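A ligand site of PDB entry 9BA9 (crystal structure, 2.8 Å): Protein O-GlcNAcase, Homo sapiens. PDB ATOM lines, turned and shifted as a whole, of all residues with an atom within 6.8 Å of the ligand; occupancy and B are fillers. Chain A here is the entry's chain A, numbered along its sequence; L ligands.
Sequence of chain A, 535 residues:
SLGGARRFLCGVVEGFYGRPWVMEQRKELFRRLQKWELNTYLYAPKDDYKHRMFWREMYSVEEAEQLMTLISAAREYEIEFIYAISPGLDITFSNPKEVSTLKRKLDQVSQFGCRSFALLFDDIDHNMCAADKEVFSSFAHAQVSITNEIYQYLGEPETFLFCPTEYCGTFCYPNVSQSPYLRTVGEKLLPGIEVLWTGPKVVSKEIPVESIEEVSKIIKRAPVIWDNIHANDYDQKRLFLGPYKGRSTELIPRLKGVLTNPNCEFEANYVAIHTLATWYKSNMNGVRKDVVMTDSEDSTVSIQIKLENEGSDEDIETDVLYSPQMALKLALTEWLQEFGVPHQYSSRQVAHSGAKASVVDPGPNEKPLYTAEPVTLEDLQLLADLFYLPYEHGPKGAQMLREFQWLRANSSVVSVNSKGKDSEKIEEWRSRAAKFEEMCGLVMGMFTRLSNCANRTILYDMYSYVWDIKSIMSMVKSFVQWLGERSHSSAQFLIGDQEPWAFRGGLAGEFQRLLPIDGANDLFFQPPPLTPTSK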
ATOM      1  N   GLY A  15     -24.912  -1.846   8.432  1.00  0.00           N
ATOM      2  CA  GLY A  15     -23.525  -1.500   8.112  1.00  0.00           C
ATOM      3  C   GLY A  15     -22.685  -1.035   9.293  1.00  0.00           C
ATOM      4  O   GLY A  15     -21.900  -0.104   9.151  1.00  0.00           O
ATOM      5  N   PHE A  16     -22.850  -1.674  10.442  1.00  0.00           N
ATOM      6  CA  PHE A  16     -22.094  -1.335  11.636  1.00  0.00           C
ATOM      7  C   PHE A  16     -20.942  -2.322  11.861  1.00  0.00           C
ATOM      8  O   PHE A  16     -20.863  -3.366  11.205  1.00  0.00           O
ATOM      9  CB  PHE A  16     -22.997  -1.300  12.872  1.00  0.00           C
ATOM     10  CG  PHE A  16     -23.913  -2.491  12.994  1.00  0.00           C
ATOM     11  CD1 PHE A  16     -25.272  -2.356  12.722  1.00  0.00           C
ATOM     12  CD2 PHE A  16     -23.425  -3.737  13.372  1.00  0.00           C
ATOM     13  CE1 PHE A  16     -26.120  -3.446  12.830  1.00  0.00           C
ATOM     14  CE2 PHE A  16     -24.273  -4.827  13.479  1.00  0.00           C
ATOM     15  CZ  PHE A  16     -25.627  -4.683  13.209  1.00  0.00           C
ATOM     16  N   TYR A  17     -20.047  -1.998  12.790  1.00  0.00           N
ATOM     17  CA  TYR A  17     -19.053  -2.956  13.254  1.00  0.00           C
ATOM     18  C   TYR A  17     -19.676  -3.776  14.376  1.00  0.00           C
ATOM     19  O   TYR A  17     -20.399  -3.226  15.216  1.00  0.00           O
ATOM     20  CB  TYR A  17     -17.799  -2.242  13.746  1.00  0.00           C
ATOM     21  CG  TYR A  17     -17.059  -1.471  12.659  1.00  0.00           C
ATOM     22  CD1 TYR A  17     -16.129  -2.110  11.842  1.00  0.00           C
ATOM     23  CD2 TYR A  17     -17.296  -0.118  12.455  1.00  0.00           C
ATOM     24  CE1 TYR A  17     -15.461  -1.408  10.854  1.00  0.00           C
ATOM     25  CE2 TYR A  17     -16.637   0.590  11.468  1.00  0.00           C
ATOM     26  CZ  TYR A  17     -15.710  -0.061  10.671  1.00  0.00           C
ATOM     27  OH  TYR A  17     -15.037   0.627   9.690  1.00  0.00           O
ATOM     28  N   ALA A  44     -24.595  -4.533   4.468  1.00  0.00           N
ATOM     29  CA  ALA A  44     -23.235  -4.007   4.596  1.00  0.00           C
ATOM     30  C   ALA A  44     -22.510  -4.357   5.912  1.00  0.00           C
ATOM     31  O   ALA A  44     -21.809  -3.532   6.481  1.00  0.00           O
ATOM     32  CB  ALA A  44     -23.274  -2.492   4.397  1.00  0.00           C
ATOM     33  N   LYS A  46     -19.904  -4.804   8.351  1.00  0.00           N
ATOM     34  CA  LYS A  46     -18.456  -4.609   8.321  1.00  0.00           C
ATOM     35  C   LYS A  46     -17.726  -5.882   8.708  1.00  0.00           C
ATOM     36  O   LYS A  46     -16.602  -6.105   8.280  1.00  0.00           O
ATOM     37  CB  LYS A  46     -18.017  -3.457   9.223  1.00  0.00           C
ATOM     38  CG  LYS A  46     -18.472  -2.073   8.768  1.00  0.00           C
ATOM     39  CD  LYS A  46     -17.515  -1.502   7.721  1.00  0.00           C
ATOM     40  CE  LYS A  46     -17.769  -0.009   7.485  1.00  0.00           C
ATOM     41  NZ  LYS A  46     -19.003   0.253   6.704  1.00  0.00           N
ATOM     42  N   LEU A 120     -18.607   0.313  -1.725  1.00  0.00           N
ATOM     43  CA  LEU A 120     -18.296   1.138  -0.570  1.00  0.00           C
ATOM     44  C   LEU A 120     -16.792   1.354  -0.379  1.00  0.00           C
ATOM     45  O   LEU A 120     -15.995   0.396  -0.384  1.00  0.00           O
ATOM     46  CB  LEU A 120     -18.914   0.548   0.711  1.00  0.00           C
ATOM     47  CG  LEU A 120     -20.370   0.061   0.646  1.00  0.00           C
ATOM     48  CD1 LEU A 120     -20.734  -0.657   1.942  1.00  0.00           C
ATOM     49  CD2 LEU A 120     -21.339   1.202   0.344  1.00  0.00           C
ATOM     50  N   ASP A 122     -15.743   3.519   2.263  1.00  0.00           N
ATOM     51  CA  ASP A 122     -15.794   4.211   3.542  1.00  0.00           C
ATOM     52  C   ASP A 122     -14.811   3.581   4.541  1.00  0.00           C
ATOM     53  O   ASP A 122     -14.564   2.369   4.498  1.00  0.00           O
ATOM     54  CB  ASP A 122     -17.225   4.212   4.099  1.00  0.00           C
ATOM     55  CG  ASP A 122     -17.767   2.800   4.386  1.00  0.00           C
ATOM     56  OD1 ASP A 122     -18.299   2.601   5.505  1.00  0.00           O
ATOM     57  OD2 ASP A 122     -17.670   1.899   3.523  1.00  0.00           O
ATOM     58  N   ASP A 123     -14.262   4.427   5.417  1.00  0.00           N
ATOM     59  CA  ASP A 123     -13.300   4.050   6.469  1.00  0.00           C
ATOM     60  C   ASP A 123     -12.044   3.337   5.931  1.00  0.00           C
ATOM     61  O   ASP A 123     -11.684   2.253   6.389  1.00  0.00           O
ATOM     62  CB  ASP A 123     -13.994   3.248   7.589  1.00  0.00           C
ATOM     63  CG  ASP A 123     -15.086   4.070   8.329  1.00  0.00           C
ATOM     64  OD1 ASP A 123     -15.840   3.467   9.134  1.00  0.00           O
ATOM     65  OD2 ASP A 123     -15.183   5.307   8.110  1.00  0.00           O
ATOM     66  N   CYS A 163     -20.403   4.601  -2.141  1.00  0.00           N
ATOM     67  CA  CYS A 163     -20.049   5.303  -0.923  1.00  0.00           C
ATOM     68  C   CYS A 163     -18.621   5.873  -0.977  1.00  0.00           C
ATOM     69  O   CYS A 163     -17.654   5.111  -1.063  1.00  0.00           O
ATOM     70  CB  CYS A 163     -20.251   4.435   0.322  1.00  0.00           C
ATOM     71  SG  CYS A 163     -20.170   5.392   1.855  1.00  0.00           S
ATOM     72  N   PRO A 164     -18.505   7.208  -0.927  1.00  0.00           N
ATOM     73  CA  PRO A 164     -17.243   7.942  -0.938  1.00  0.00           C
ATOM     74  C   PRO A 164     -16.294   7.520   0.199  1.00  0.00           C
ATOM     75  O   PRO A 164     -16.685   6.810   1.125  1.00  0.00           O
ATOM     76  CB  PRO A 164     -17.670   9.398  -0.700  1.00  0.00           C
ATOM     77  CG  PRO A 164     -19.090   9.454  -1.148  1.00  0.00           C
ATOM     78  CD  PRO A 164     -19.664   8.116  -0.819  1.00  0.00           C
ATOM     79  N   TYR A 167     -16.967  10.711   3.018  1.00  0.00           N
ATOM     80  CA  TYR A 167     -18.401  10.428   3.016  1.00  0.00           C
ATOM     81  C   TYR A 167     -19.260  11.359   3.882  1.00  0.00           C
ATOM     82  O   TYR A 167     -20.468  11.157   3.983  1.00  0.00           O
ATOM     83  CB  TYR A 167     -18.677   8.962   3.337  1.00  0.00           C
ATOM     84  CG  TYR A 167     -18.295   8.483   4.725  1.00  0.00           C
ATOM     85  CD1 TYR A 167     -19.044   8.854   5.848  1.00  0.00           C
ATOM     86  CD2 TYR A 167     -17.229   7.620   4.911  1.00  0.00           C
ATOM     87  CE1 TYR A 167     -18.716   8.394   7.111  1.00  0.00           C
ATOM     88  CE2 TYR A 167     -16.885   7.151   6.162  1.00  0.00           C
ATOM     89  CZ  TYR A 167     -17.626   7.543   7.257  1.00  0.00           C
ATOM     90  OH  TYR A 167     -17.266   7.065   8.495  1.00  0.00           O
ATOM     91  N   LEU A 196     -23.730   7.987  -1.424  1.00  0.00           N
ATOM     92  CA  LEU A 196     -24.102   7.951  -0.015  1.00  0.00           C
ATOM     93  C   LEU A 196     -23.410   9.068   0.771  1.00  0.00           C
ATOM     94  O   LEU A 196     -22.252   9.405   0.509  1.00  0.00           O
ATOM     95  CB  LEU A 196     -23.831   6.572   0.596  1.00  0.00           C
ATOM     96  CG  LEU A 196     -24.753   5.456   0.070  1.00  0.00           C
ATOM     97  CD1 LEU A 196     -24.087   4.092   0.148  1.00  0.00           C
ATOM     98  CD2 LEU A 196     -26.120   5.456   0.753  1.00  0.00           C
ATOM     99  N   TRP A 197     -24.153   9.658   1.708  1.00  0.00           N
ATOM    100  CA  TRP A 197     -23.689  10.804   2.486  1.00  0.00           C
ATOM    101  C   TRP A 197     -24.297  10.665   3.881  1.00  0.00           C
ATOM    102  O   TRP A 197     -25.429  10.207   4.006  1.00  0.00           O
ATOM    103  CB  TRP A 197     -24.164  12.088   1.808  1.00  0.00           C
ATOM    104  CG  TRP A 197     -23.645  13.379   2.397  1.00  0.00           C
ATOM    105  CD1 TRP A 197     -24.372  14.328   3.063  1.00  0.00           C
ATOM    106  CD2 TRP A 197     -22.303  13.885   2.322  1.00  0.00           C
ATOM    107  NE1 TRP A 197     -23.558  15.380   3.428  1.00  0.00           N
ATOM    108  CE2 TRP A 197     -22.289  15.130   2.985  1.00  0.00           C
ATOM    109  CE3 TRP A 197     -21.113  13.387   1.765  1.00  0.00           C
ATOM    110  CZ2 TRP A 197     -21.117  15.896   3.106  1.00  0.00           C
ATOM    111  CZ3 TRP A 197     -19.949  14.156   1.897  1.00  0.00           C
ATOM    112  CH2 TRP A 197     -19.971  15.400   2.553  1.00  0.00           C
ATOM    113  N   THR A 198     -23.555  11.058   4.920  1.00  0.00           N
ATOM    114  CA  THR A 198     -24.048  10.922   6.296  1.00  0.00           C
ATOM    115  C   THR A 198     -24.359  12.266   6.967  1.00  0.00           C
ATOM    116  O   THR A 198     -24.806  12.304   8.128  1.00  0.00           O
ATOM    117  CB  THR A 198     -23.096  10.118   7.216  1.00  0.00           C
ATOM    118  OG1 THR A 198     -22.023  10.954   7.657  1.00  0.00           O
ATOM    119  CG2 THR A 198     -22.524   8.891   6.509  1.00  0.00           C
ATOM    120  N   VAL A 202     -19.910  11.965  10.824  1.00  0.00           N
ATOM    121  CA  VAL A 202     -20.273  10.542  10.783  1.00  0.00           C
ATOM    122  C   VAL A 202     -21.620  10.331  11.480  1.00  0.00           C
ATOM    123  O   VAL A 202     -22.558   9.788  10.883  1.00  0.00           O
ATOM    124  CB  VAL A 202     -19.212   9.646  11.462  1.00  0.00           C
ATOM    125  CG1 VAL A 202     -19.624   8.183  11.410  1.00  0.00           C
ATOM    126  CG2 VAL A 202     -17.844   9.841  10.812  1.00  0.00           C
ATOM    127  N   VAL A 203     -21.702  10.776  12.732  1.00  0.00           N
ATOM    128  CA  VAL A 203     -22.959  10.788  13.478  1.00  0.00           C
ATOM    129  C   VAL A 203     -23.446  12.244  13.550  1.00  0.00           C
ATOM    130  O   VAL A 203     -23.011  13.018  14.406  1.00  0.00           O
ATOM    131  CB  VAL A 203     -22.771  10.188  14.897  1.00  0.00           C
ATOM    132  CG1 VAL A 203     -24.098  10.103  15.627  1.00  0.00           C
ATOM    133  CG2 VAL A 203     -22.138   8.810  14.804  1.00  0.00           C
ATOM    134  N   TRP A 226     -26.938   7.944   4.469  1.00  0.00           N
ATOM    135  CA  TRP A 226     -26.602   6.792   5.265  1.00  0.00           C
ATOM    136  C   TRP A 226     -26.594   7.370   6.677  1.00  0.00           C
ATOM    137  O   TRP A 226     -25.597   7.937   7.111  1.00  0.00           O
ATOM    138  CB  TRP A 226     -25.228   6.234   4.848  1.00  0.00           C
ATOM    139  CG  TRP A 226     -24.600   5.158   5.740  1.00  0.00           C
ATOM    140  CD1 TRP A 226     -24.552   5.134   7.108  1.00  0.00           C
ATOM    141  CD2 TRP A 226     -23.890   3.981   5.301  1.00  0.00           C
ATOM    142  NE1 TRP A 226     -23.884   4.022   7.548  1.00  0.00           N
ATOM    143  CE2 TRP A 226     -23.463   3.296   6.459  1.00  0.00           C
ATOM    144  CE3 TRP A 226     -23.580   3.448   4.051  1.00  0.00           C
ATOM    145  CZ2 TRP A 226     -22.736   2.092   6.399  1.00  0.00           C
ATOM    146  CZ3 TRP A 226     -22.857   2.259   3.984  1.00  0.00           C
ATOM    147  CH2 TRP A 226     -22.450   1.596   5.155  1.00  0.00           C
ATOM    148  N   ASP A 227     -27.732   7.280   7.372  1.00  0.00           N
ATOM    149  CA  ASP A 227     -27.869   7.990   8.629  1.00  0.00           C
ATOM    150  C   ASP A 227     -27.372   7.180   9.806  1.00  0.00           C
ATOM    151  O   ASP A 227     -27.793   6.042   9.996  1.00  0.00           O
ATOM    152  CB  ASP A 227     -29.309   8.460   8.869  1.00  0.00           C
ATOM    153  CG  ASP A 227     -29.373   9.688   9.779  1.00  0.00           C
ATOM    154  OD1 ASP A 227     -28.538   9.825  10.710  1.00  0.00           O
ATOM    155  OD2 ASP A 227     -30.281  10.530   9.557  1.00  0.00           O
ATOM    156  N   ASN A 228     -26.486   7.787  10.587  1.00  0.00           N
ATOM    157  CA  ASN A 228     -25.897   7.123  11.735  1.00  0.00           C
ATOM    158  C   ASN A 228     -26.403   7.661  13.061  1.00  0.00           C
ATOM    159  O   ASN A 228     -25.744   7.512  14.082  1.00  0.00           O
ATOM    160  CB  ASN A 228     -24.371   7.215  11.687  1.00  0.00           C
ATOM    161  CG  ASN A 228     -23.784   6.430  10.536  1.00  0.00           C
ATOM    162  OD1 ASN A 228     -24.228   5.318  10.236  1.00  0.00           O
ATOM    163  ND2 ASN A 228     -22.776   6.988   9.898  1.00  0.00           N
ATOM    164  N   ALA A 231     -26.734   4.603  15.539  1.00  0.00           N
ATOM    165  CA  ALA A 231     -25.665   3.628  15.642  1.00  0.00           C
ATOM    166  C   ALA A 231     -25.005   3.674  17.010  1.00  0.00           C
ATOM    167  O   ALA A 231     -24.873   4.739  17.592  1.00  0.00           O
ATOM    168  CB  ALA A 231     -24.630   3.842  14.556  1.00  0.00           C
ATOM    169  N   ASN A 232     -24.608   2.517  17.527  1.00  0.00           N
ATOM    170  CA  ASN A 232     -23.905   2.439  18.806  1.00  0.00           C
ATOM    171  C   ASN A 232     -22.637   1.578  18.775  1.00  0.00           C
ATOM    172  O   ASN A 232     -22.222   1.048  19.800  1.00  0.00           O
ATOM    173  CB  ASN A 232     -24.843   1.945  19.911  1.00  0.00           C
ATOM    174  CG  ASN A 232     -25.321   0.535  19.679  1.00  0.00           C
ATOM    175  OD1 ASN A 232     -25.281   0.024  18.554  1.00  0.00           O
ATOM    176  ND2 ASN A 232     -25.786  -0.118  20.739  1.00  0.00           N
ATOM    177  N   ASP A 233     -21.999   1.450  17.609  1.00  0.00           N
ATOM    178  CA  ASP A 233     -20.831   0.594  17.515  1.00  0.00           C
ATOM    179  C   ASP A 233     -19.530   1.244  18.017  1.00  0.00           C
ATOM    180  O   ASP A 233     -18.466   0.621  17.959  1.00  0.00           O
ATOM    181  CB  ASP A 233     -20.673  -0.049  16.133  1.00  0.00           C
ATOM    182  CG  ASP A 233     -20.570   0.962  15.003  1.00  0.00           C
ATOM    183  OD1 ASP A 233     -20.115   0.576  13.911  1.00  0.00           O
ATOM    184  OD2 ASP A 233     -20.941   2.144  15.194  1.00  0.00           O
ATOM    185  N   TYR A 234     -19.597   2.468  18.522  1.00  0.00           N
ATOM    186  CA  TYR A 234     -18.420   3.102  19.122  1.00  0.00           C
ATOM    187  C   TYR A 234     -18.173   2.619  20.550  1.00  0.00           C
ATOM    188  O   TYR A 234     -18.997   2.842  21.439  1.00  0.00           O
ATOM    189  CB  TYR A 234     -18.395   4.644  19.001  1.00  0.00           C
ATOM    190  CG  TYR A 234     -19.728   5.368  18.890  1.00  0.00           C
ATOM    191  CD1 TYR A 234     -20.098   6.319  19.841  1.00  0.00           C
ATOM    192  CD2 TYR A 234     -20.580   5.158  17.810  1.00  0.00           C
ATOM    193  CE1 TYR A 234     -21.292   7.019  19.735  1.00  0.00           C
ATOM    194  CE2 TYR A 234     -21.785   5.842  17.703  1.00  0.00           C
ATOM    195  CZ  TYR A 234     -22.132   6.767  18.660  1.00  0.00           C
ATOM    196  OH  TYR A 234     -23.323   7.454  18.553  1.00  0.00           O
ATOM    197  N   ASN A 261     -28.577   3.350   9.867  1.00  0.00           N
ATOM    198  CA  ASN A 261     -27.629   2.380  10.393  1.00  0.00           C
ATOM    199  C   ASN A 261     -27.773   2.307  11.911  1.00  0.00           C
ATOM    200  O   ASN A 261     -27.049   2.990  12.633  1.00  0.00           O
ATOM    201  CB  ASN A 261     -26.216   2.785  10.008  1.00  0.00           C
ATOM    202  CG  ASN A 261     -25.181   1.691  10.260  1.00  0.00           C
ATOM    203  OD1 ASN A 261     -25.424   0.517   9.987  1.00  0.00           O
ATOM    204  ND2 ASN A 261     -24.025   2.089  10.773  1.00  0.00           N
HETATM  205  C1  LIG L   1     -17.913   3.526  14.031  1.00  0.00           C
HETATM  206  C2  LIG L   1     -19.288   5.493  14.759  1.00  0.00           C
HETATM  207  C3  LIG L   1     -20.038   2.174  10.389  1.00  0.00           C
HETATM  208  C4  LIG L   1     -17.889   4.996  14.428  1.00  0.00           C
HETATM  209  C5  LIG L   1     -20.519   5.159   6.865  1.00  0.00           C
HETATM  210  C6  LIG L   1     -20.094   3.454   8.617  1.00  0.00           C
HETATM  211  C7  LIG L   1     -20.738   3.222  10.923  1.00  0.00           C
HETATM  212  C8  LIG L   1     -20.260   5.173  13.615  1.00  0.00           C
HETATM  213  C9  LIG L   1     -18.910   3.278  12.908  1.00  0.00           C
HETATM  214  C10 LIG L   1     -20.194   5.388   5.412  1.00  0.00           C
HETATM  215  C11 LIG L   1     -21.278   3.404  12.311  1.00  0.00           C
HETATM  216  N1  LIG L   1     -19.672   2.300   9.062  1.00  0.00           N
HETATM  217  N2  LIG L   1     -20.255   3.727  13.320  1.00  0.00           N
HETATM  218  N3  LIG L   1     -19.965   3.959   7.355  1.00  0.00           N
HETATM  219  O1  LIG L   1     -21.179   5.966   7.518  1.00  0.00           O
HETATM  220  S1  LIG L   1     -20.970   4.436   9.723  1.00  0.00           S
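The side-chain carboxylate (OD2) of Asp 233 lies within salt-bridge range of a nitrogen (N2) of the ligand.
OD1 of Asp 122 sits at hydrogen-bond distance from N3 of the ligand (2.8 Å).
The side-chain amide nitrogen (ND2) of Asn 228 lies within hydrogen-bond range of an oxygen (O1) of the ligand.
The side-chain amino group of Lys 46 sits at hydrogen-bond distance from a nitrogen (N1) of the ligand (3.2 Å).
The indole nitrogen (NE1) of Trp 226 lies within hydrogen-bond range of an oxygen (O1) of the ligand, 3.3 Å away.
The side-chain carboxylate (OD1) of Asp 233 is in hydrogen-bond range of the backbone NH (N) of Tyr 17, at 2.8 Å.
The side-chain amide oxygen of Asn 228 sits at hydrogen-bond distance from the indole nitrogen of Trp 226 (3.0 Å).
The backbone NH (N) of Trp 226 lies within hydrogen-bond range of the backbone carbonyl oxygen (O) of Trp 197 (2.8 Å).
OG1 of Thr 198 sits at hydrogen-bond distance from O of Val 202, 3.5 Å away.
O of Asn 261 lies close to N of Ala 231 (3.3 Å).
The side-chain amide oxygen of Asn 261 sits at hydrogen-bond distance from the backbone NH of Phe 16 (3.4 Å).
The side-chain carboxylate of Asp 123 lies within hydrogen-bond range of the side-chain hydroxyl of Tyr 167 (2.8 Å).
OH of Tyr 17 lies within hydrogen-bond range of OD1 of Asp 123 (3.0 Å).
O of Gly 15 sits close to N1 of the ligand (3.3 Å).
Tyr 17 touches the ligand (CD2 to C9, 3.8 Å).
SG of Cys 163 touches C10 of the ligand, at 3.6 Å.
Tyr 167 touches the ligand (CE1 to O1, 3.5 Å).
CG2 of Thr 198 touches O1 of the ligand (3.4 Å).
Val 202 touches the ligand (CG1 to C8, 3.8 Å).
Tyr 234 touches the ligand (CD2 to C2, 3.3 Å).
ND2 of Asn 261 touches C11 of the ligand, at 3.4 Å.
Hydrophobic or aromatic side chains within 4 Å of the ligand: Tyr 17, Tyr 167, Val 202, Trp 226 and Tyr 234.
13 residues have an atom within 4 Å of the ligand: Gly 15, Tyr 17, Lys 46, Asp 122, Cys 163, Tyr 167, Thr 198, Val 202, Trp 226, Asn 228, Asp 233, Tyr 234 and Asn 261.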
